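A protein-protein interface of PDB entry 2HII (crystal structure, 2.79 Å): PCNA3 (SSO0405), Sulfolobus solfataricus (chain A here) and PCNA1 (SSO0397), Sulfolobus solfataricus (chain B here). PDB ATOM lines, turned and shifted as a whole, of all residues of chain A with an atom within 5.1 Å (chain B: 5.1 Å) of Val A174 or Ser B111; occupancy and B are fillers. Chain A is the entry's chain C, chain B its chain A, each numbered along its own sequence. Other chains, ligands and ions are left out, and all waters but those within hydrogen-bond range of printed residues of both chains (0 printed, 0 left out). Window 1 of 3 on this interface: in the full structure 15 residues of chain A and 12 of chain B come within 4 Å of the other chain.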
ATOM      1  N   ALA A 142      -4.351   7.648 -18.896  1.00  0.00           N
ATOM      2  CA  ALA A 142      -3.954   8.021 -17.550  1.00  0.00           C
ATOM      3  C   ALA A 142      -2.631   7.380 -17.192  1.00  0.00           C
ATOM      4  O   ALA A 142      -1.656   8.069 -16.895  1.00  0.00           O
ATOM      5  CB  ALA A 142      -5.001   7.608 -16.564  1.00  0.00           C
ATOM      6  N   GLU A 145       0.367   8.399 -19.539  1.00  0.00           N
ATOM      7  CA  GLU A 145       0.831   9.737 -19.148  1.00  0.00           C
ATOM      8  C   GLU A 145       1.775   9.747 -17.952  1.00  0.00           C
ATOM      9  O   GLU A 145       2.827  10.382 -17.978  1.00  0.00           O
ATOM     10  CB  GLU A 145      -0.368  10.627 -18.822  1.00  0.00           C
ATOM     11  CG  GLU A 145      -1.056  11.201 -20.027  1.00  0.00           C
ATOM     12  CD  GLU A 145      -2.404  11.774 -19.674  1.00  0.00           C
ATOM     13  OE1 GLU A 145      -2.449  12.743 -18.891  1.00  0.00           O
ATOM     14  OE2 GLU A 145      -3.424  11.254 -20.180  1.00  0.00           O
ATOM     15  N   VAL A 146       1.371   9.038 -16.907  1.00  0.00           N
ATOM     16  CA  VAL A 146       2.041   9.055 -15.617  1.00  0.00           C
ATOM     17  C   VAL A 146       3.332   8.248 -15.670  1.00  0.00           C
ATOM     18  O   VAL A 146       4.363   8.674 -15.157  1.00  0.00           O
ATOM     19  CB  VAL A 146       1.092   8.508 -14.524  1.00  0.00           C
ATOM     20  CG1 VAL A 146       1.786   8.418 -13.184  1.00  0.00           C
ATOM     21  CG2 VAL A 146      -0.137   9.394 -14.406  1.00  0.00           C
ATOM     22  N   ILE A 162     -11.329  10.029  -8.383  1.00  0.00           N
ATOM     23  CA  ILE A 162     -10.156   9.130  -8.356  1.00  0.00           C
ATOM     24  C   ILE A 162      -9.027   9.817  -9.097  1.00  0.00           C
ATOM     25  O   ILE A 162      -9.220  10.400 -10.179  1.00  0.00           O
ATOM     26  CB  ILE A 162     -10.372   7.781  -9.102  1.00  0.00           C
ATOM     27  CG1 ILE A 162     -11.842   7.444  -9.249  1.00  0.00           C
ATOM     28  CG2 ILE A 162      -9.574   6.632  -8.484  1.00  0.00           C
ATOM     29  CD1 ILE A 162     -12.364   7.885 -10.559  1.00  0.00           C
ATOM     30  N   LEU A 163      -7.839   9.745  -8.529  1.00  0.00           N
ATOM     31  CA  LEU A 163      -6.714  10.379  -9.169  1.00  0.00           C
ATOM     32  C   LEU A 163      -5.746   9.306  -9.549  1.00  0.00           C
ATOM     33  O   LEU A 163      -5.545   8.365  -8.810  1.00  0.00           O
ATOM     34  CB  LEU A 163      -6.040  11.412  -8.252  1.00  0.00           C
ATOM     35  CG  LEU A 163      -6.904  12.446  -7.511  1.00  0.00           C
ATOM     36  CD1 LEU A 163      -6.058  13.250  -6.556  1.00  0.00           C
ATOM     37  CD2 LEU A 163      -7.638  13.359  -8.441  1.00  0.00           C
ATOM     38  N   ILE A 164      -5.177   9.421 -10.732  1.00  0.00           N
ATOM     39  CA  ILE A 164      -4.024   8.631 -11.057  1.00  0.00           C
ATOM     40  C   ILE A 164      -2.905   9.636 -11.175  1.00  0.00           C
ATOM     41  O   ILE A 164      -2.997  10.596 -11.935  1.00  0.00           O
ATOM     42  CB  ILE A 164      -4.220   7.787 -12.317  1.00  0.00           C
ATOM     43  CG1 ILE A 164      -5.227   6.663 -12.028  1.00  0.00           C
ATOM     44  CG2 ILE A 164      -2.907   7.198 -12.743  1.00  0.00           C
ATOM     45  CD1 ILE A 164      -5.414   5.644 -13.156  1.00  0.00           C
ATOM     46  N   LYS A 165      -1.867   9.442 -10.376  1.00  0.00           N
ATOM     47  CA  LYS A 165      -0.862  10.470 -10.228  1.00  0.00           C
ATOM     48  C   LYS A 165       0.553   9.955 -10.091  1.00  0.00           C
ATOM     49  O   LYS A 165       0.770   8.792  -9.744  1.00  0.00           O
ATOM     50  CB  LYS A 165      -1.215  11.423  -9.080  1.00  0.00           C
ATOM     51  CG  LYS A 165      -1.349  10.807  -7.715  1.00  0.00           C
ATOM     52  CD  LYS A 165      -2.475  11.486  -6.954  1.00  0.00           C
ATOM     53  CE  LYS A 165      -2.114  12.881  -6.471  1.00  0.00           C
ATOM     54  NZ  LYS A 165      -1.449  12.823  -5.140  1.00  0.00           N
ATOM     55  N   VAL A 172       2.310  14.876 -11.702  1.00  0.00           N
ATOM     56  CA  VAL A 172       1.255  14.719 -12.680  1.00  0.00           C
ATOM     57  C   VAL A 172       0.081  14.120 -11.959  1.00  0.00           C
ATOM     58  O   VAL A 172       0.240  13.236 -11.147  1.00  0.00           O
ATOM     59  CB  VAL A 172       1.664  13.765 -13.807  1.00  0.00           C
ATOM     60  CG1 VAL A 172       0.503  13.505 -14.714  1.00  0.00           C
ATOM     61  CG2 VAL A 172       2.790  14.340 -14.602  1.00  0.00           C
ATOM     62  N   GLU A 173      -1.106  14.597 -12.262  1.00  0.00           N
ATOM     63  CA  GLU A 173      -2.291  14.104 -11.608  1.00  0.00           C
ATOM     64  C   GLU A 173      -3.416  14.073 -12.642  1.00  0.00           C
ATOM     65  O   GLU A 173      -3.784  15.108 -13.206  1.00  0.00           O
ATOM     66  CB  GLU A 173      -2.596  14.999 -10.413  1.00  0.00           C
ATOM     67  CG  GLU A 173      -3.998  14.929  -9.889  1.00  0.00           C
ATOM     68  CD  GLU A 173      -4.336  16.137  -9.049  1.00  0.00           C
ATOM     69  OE1 GLU A 173      -3.510  16.491  -8.171  1.00  0.00           O
ATOM     70  OE2 GLU A 173      -5.423  16.726  -9.279  1.00  0.00           O
ATOM     71  N   VAL A 174      -3.914  12.870 -12.920  1.00  0.00           N
ATOM     72  CA  VAL A 174      -4.989  12.657 -13.888  1.00  0.00           C
ATOM     73  C   VAL A 174      -6.260  12.356 -13.114  1.00  0.00           C
ATOM     74  O   VAL A 174      -6.366  11.328 -12.478  1.00  0.00           O
ATOM     75  CB  VAL A 174      -4.663  11.486 -14.848  1.00  0.00           C
ATOM     76  CG1 VAL A 174      -5.635  11.441 -15.996  1.00  0.00           C
ATOM     77  CG2 VAL A 174      -3.246  11.605 -15.382  1.00  0.00           C
ATOM     78  N   GLU A 175      -7.223  13.257 -13.167  1.00  0.00           N
ATOM     79  CA  GLU A 175      -8.394  13.159 -12.313  1.00  0.00           C
ATOM     80  C   GLU A 175      -9.616  12.674 -13.073  1.00  0.00           C
ATOM     81  O   GLU A 175      -9.917  13.169 -14.158  1.00  0.00           O
ATOM     82  CB  GLU A 175      -8.692  14.521 -11.675  1.00  0.00           C
ATOM     83  CG  GLU A 175      -9.994  14.591 -10.899  1.00  0.00           C
ATOM     84  CD  GLU A 175     -10.159  15.893 -10.161  1.00  0.00           C
ATOM     85  OE1 GLU A 175     -11.148  16.611 -10.439  1.00  0.00           O
ATOM     86  OE2 GLU A 175      -9.296  16.204  -9.309  1.00  0.00           O
ATOM     87  N   PHE A 176     -10.323  11.715 -12.490  1.00  0.00           N
ATOM     88  CA  PHE A 176     -11.650  11.390 -12.960  1.00  0.00           C
ATOM     89  C   PHE A 176     -12.622  11.729 -11.834  1.00  0.00           C
ATOM     90  O   PHE A 176     -12.541  11.147 -10.746  1.00  0.00           O
ATOM     91  CB  PHE A 176     -11.758   9.911 -13.347  1.00  0.00           C
ATOM     92  CG  PHE A 176     -10.749   9.455 -14.373  1.00  0.00           C
ATOM     93  CD1 PHE A 176      -9.537   8.896 -13.983  1.00  0.00           C
ATOM     94  CD2 PHE A 176     -11.025   9.541 -15.731  1.00  0.00           C
ATOM     95  CE1 PHE A 176      -8.603   8.458 -14.938  1.00  0.00           C
ATOM     96  CE2 PHE A 176     -10.088   9.098 -16.687  1.00  0.00           C
ATOM     97  CZ  PHE A 176      -8.881   8.561 -16.285  1.00  0.00           C
ATOM     98  N   ILE B 100       0.332  23.257 -16.040  1.00  0.00           N
ATOM     99  CA  ILE B 100      -0.335  22.983 -17.290  1.00  0.00           C
ATOM    100  C   ILE B 100      -1.473  22.020 -16.996  1.00  0.00           C
ATOM    101  O   ILE B 100      -1.251  20.966 -16.406  1.00  0.00           O
ATOM    102  CB  ILE B 100       0.618  22.374 -18.338  1.00  0.00           C
ATOM    103  CG1 ILE B 100       1.685  23.405 -18.741  1.00  0.00           C
ATOM    104  CG2 ILE B 100      -0.174  21.899 -19.552  1.00  0.00           C
ATOM    105  CD1 ILE B 100       2.622  22.964 -19.846  1.00  0.00           C
ATOM    106  N   ILE B 101      -2.694  22.383 -17.383  1.00  0.00           N
ATOM    107  CA  ILE B 101      -3.807  21.454 -17.245  1.00  0.00           C
ATOM    108  C   ILE B 101      -4.589  21.235 -18.544  1.00  0.00           C
ATOM    109  O   ILE B 101      -5.021  22.186 -19.195  1.00  0.00           O
ATOM    110  CB  ILE B 101      -4.748  21.776 -16.027  1.00  0.00           C
ATOM    111  CG1 ILE B 101      -6.046  22.444 -16.454  1.00  0.00           C
ATOM    112  CG2 ILE B 101      -4.048  22.592 -14.920  1.00  0.00           C
ATOM    113  CD1 ILE B 101      -7.101  22.297 -15.404  1.00  0.00           C
ATOM    114  N   ILE B 102      -4.739  19.959 -18.902  1.00  0.00           N
ATOM    115  CA  ILE B 102      -5.424  19.514 -20.113  1.00  0.00           C
ATOM    116  C   ILE B 102      -6.657  18.710 -19.728  1.00  0.00           C
ATOM    117  O   ILE B 102      -6.634  17.966 -18.741  1.00  0.00           O
ATOM    118  CB  ILE B 102      -4.520  18.585 -20.941  1.00  0.00           C
ATOM    119  CG1 ILE B 102      -3.157  19.228 -21.205  1.00  0.00           C
ATOM    120  CG2 ILE B 102      -5.170  18.218 -22.241  1.00  0.00           C
ATOM    121  CD1 ILE B 102      -2.068  18.755 -20.253  1.00  0.00           C
ATOM    122  N   ALA B 109     -10.818  12.999 -18.424  1.00  0.00           N
ATOM    123  CA  ALA B 109      -9.541  12.954 -17.748  1.00  0.00           C
ATOM    124  C   ALA B 109      -8.868  14.320 -17.676  1.00  0.00           C
ATOM    125  O   ALA B 109      -8.346  14.811 -18.671  1.00  0.00           O
ATOM    126  CB  ALA B 109      -8.640  11.954 -18.462  1.00  0.00           C
ATOM    127  N   LYS B 110      -8.864  14.922 -16.490  1.00  0.00           N
ATOM    128  CA  LYS B 110      -8.139  16.167 -16.252  1.00  0.00           C
ATOM    129  C   LYS B 110      -6.716  15.842 -15.811  1.00  0.00           C
ATOM    130  O   LYS B 110      -6.469  15.476 -14.669  1.00  0.00           O
ATOM    131  CB  LYS B 110      -8.885  17.024 -15.213  1.00  0.00           C
ATOM    132  CG  LYS B 110      -8.208  18.328 -14.781  1.00  0.00           C
ATOM    133  CD  LYS B 110      -9.228  19.344 -14.236  1.00  0.00           C
ATOM    134  CE  LYS B 110      -9.676  19.084 -12.790  1.00  0.00           C
ATOM    135  NZ  LYS B 110      -8.828  19.775 -11.789  1.00  0.00           N
ATOM    136  N   SER B 111      -5.784  15.944 -16.742  1.00  0.00           N
ATOM    137  CA  SER B 111      -4.375  15.808 -16.405  1.00  0.00           C
ATOM    138  C   SER B 111      -3.739  17.174 -16.190  1.00  0.00           C
ATOM    139  O   SER B 111      -3.672  18.005 -17.105  1.00  0.00           O
ATOM    140  CB  SER B 111      -3.605  14.993 -17.443  1.00  0.00           C
ATOM    141  OG  SER B 111      -4.291  14.919 -18.674  1.00  0.00           O
ATOM    142  N   THR B 112      -3.293  17.400 -14.958  1.00  0.00           N
ATOM    143  CA  THR B 112      -2.644  18.643 -14.601  1.00  0.00           C
ATOM    144  C   THR B 112      -1.163  18.360 -14.407  1.00  0.00           C
ATOM    145  O   THR B 112      -0.801  17.422 -13.706  1.00  0.00           O
ATOM    146  CB  THR B 112      -3.278  19.322 -13.339  1.00  0.00           C
ATOM    147  OG1 THR B 112      -2.577  18.930 -12.161  1.00  0.00           O
ATOM    148  CG2 THR B 112      -4.768  18.980 -13.184  1.00  0.00           C
ATOM    149  N   ILE B 113      -0.319  19.160 -15.059  1.00  0.00           N
ATOM    150  CA  ILE B 113       1.135  18.997 -15.005  1.00  0.00           C
ATOM    151  C   ILE B 113       1.800  20.144 -14.258  1.00  0.00           C
ATOM    152  O   ILE B 113       1.667  21.311 -14.633  1.00  0.00           O
ATOM    153  CB  ILE B 113       1.779  18.906 -16.419  1.00  0.00           C
ATOM    154  CG1 ILE B 113       0.924  18.081 -17.394  1.00  0.00           C
ATOM    155  CG2 ILE B 113       3.226  18.412 -16.330  1.00  0.00           C
ATOM    156  CD1 ILE B 113       0.572  16.666 -16.933  1.00  0.00           C
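Of the printed residues of chain B, Val A174 touches Ala B109 (3.9 Å), Lys B110 (3.3 Å) and Ser B111 (3.98 Å). Of the printed residues of chain A, Ser B111 touches Glu A145 (2.9 Å), Glu A173 (3.3 Å) and Val A174 (3.98 Å). Printed residues of chain B within 4 Å of Glu A175: Ala B109 and Lys B110. Of the printed residues of chain A, Thr B112 touches Val A172 and Glu A173. Printed residues of chain B within 4 Å of Val A172: Thr B112 and Ile B113. Printed residues of chain A within 4 Å of Ile B113: Val A172. Ile A162 touches none of the printed residues of chain B. The nearest printed residue of chain B that does not touch Val A174 is Thr B112 (5.0 Å).
Of the 12 printed residues of chain A, 6 touch a printed residue of chain B. Printed residues of chain A that touch a printed residue of chain B: Glu A145, Val A172, Glu A173, Val A174, Glu A175 and Phe A176. Hydrophobic or aromatic side chains of chain A that line the printed part of chain B: Val A172, Val A174 and Phe A176. Printed residues of chain B that touch a printed residue of chain A: Ala B109, Lys B110, Ser B111, Thr B112 and Ile B113. Hydrophobic or aromatic side chains of chain B within 4 Å of the printed part of chain A: Ala B109 and Ile B113. Among the printed residues, no Asp or Glu carboxylate lies within 4 Å of a Lys or Arg side-chain nitrogen of the other chain.
O of Lys B110 sits at hydrogen-bond distance from N of Glu A175, 2.8 Å away. OG of Ser B111 is in hydrogen-bond range of OE1 of Glu A145, at 2.9 Å. The backbone carbonyl oxygen (O) of Glu A173 lies within hydrogen-bond range of the backbone NH (N) of Thr B112, 2.9 Å away. O of Lys B110 sits close to O of Glu A173.
The backbone carbonyl oxygen (O) of Ile B100 lies within hydrogen-bond range of the backbone NH (N) of Ile B113, at 2.4 Å. The backbone carbonyl oxygen of Ser B111 sits at hydrogen-bond distance from the backbone NH of Ile B102 (2.9 Å). N of Phe A176 sits at hydrogen-bond distance from O of Ile A162 (2.9 Å). The backbone carbonyl oxygen (O) of Ile A164 sits at hydrogen-bond distance from the backbone NH (N) of Val A174 (2.6 Å).
Among the printed residues, pairs that only touch across the chains: Val A172 with Thr B112, Val A172 with Ile B113, Glu A173 with Ser B111, Val A174 with Ala B109, Val A174 with Lys B110, Val A174 with Ser B111, Glu A175 with Ala B109 and Phe A176 with Ala B109.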
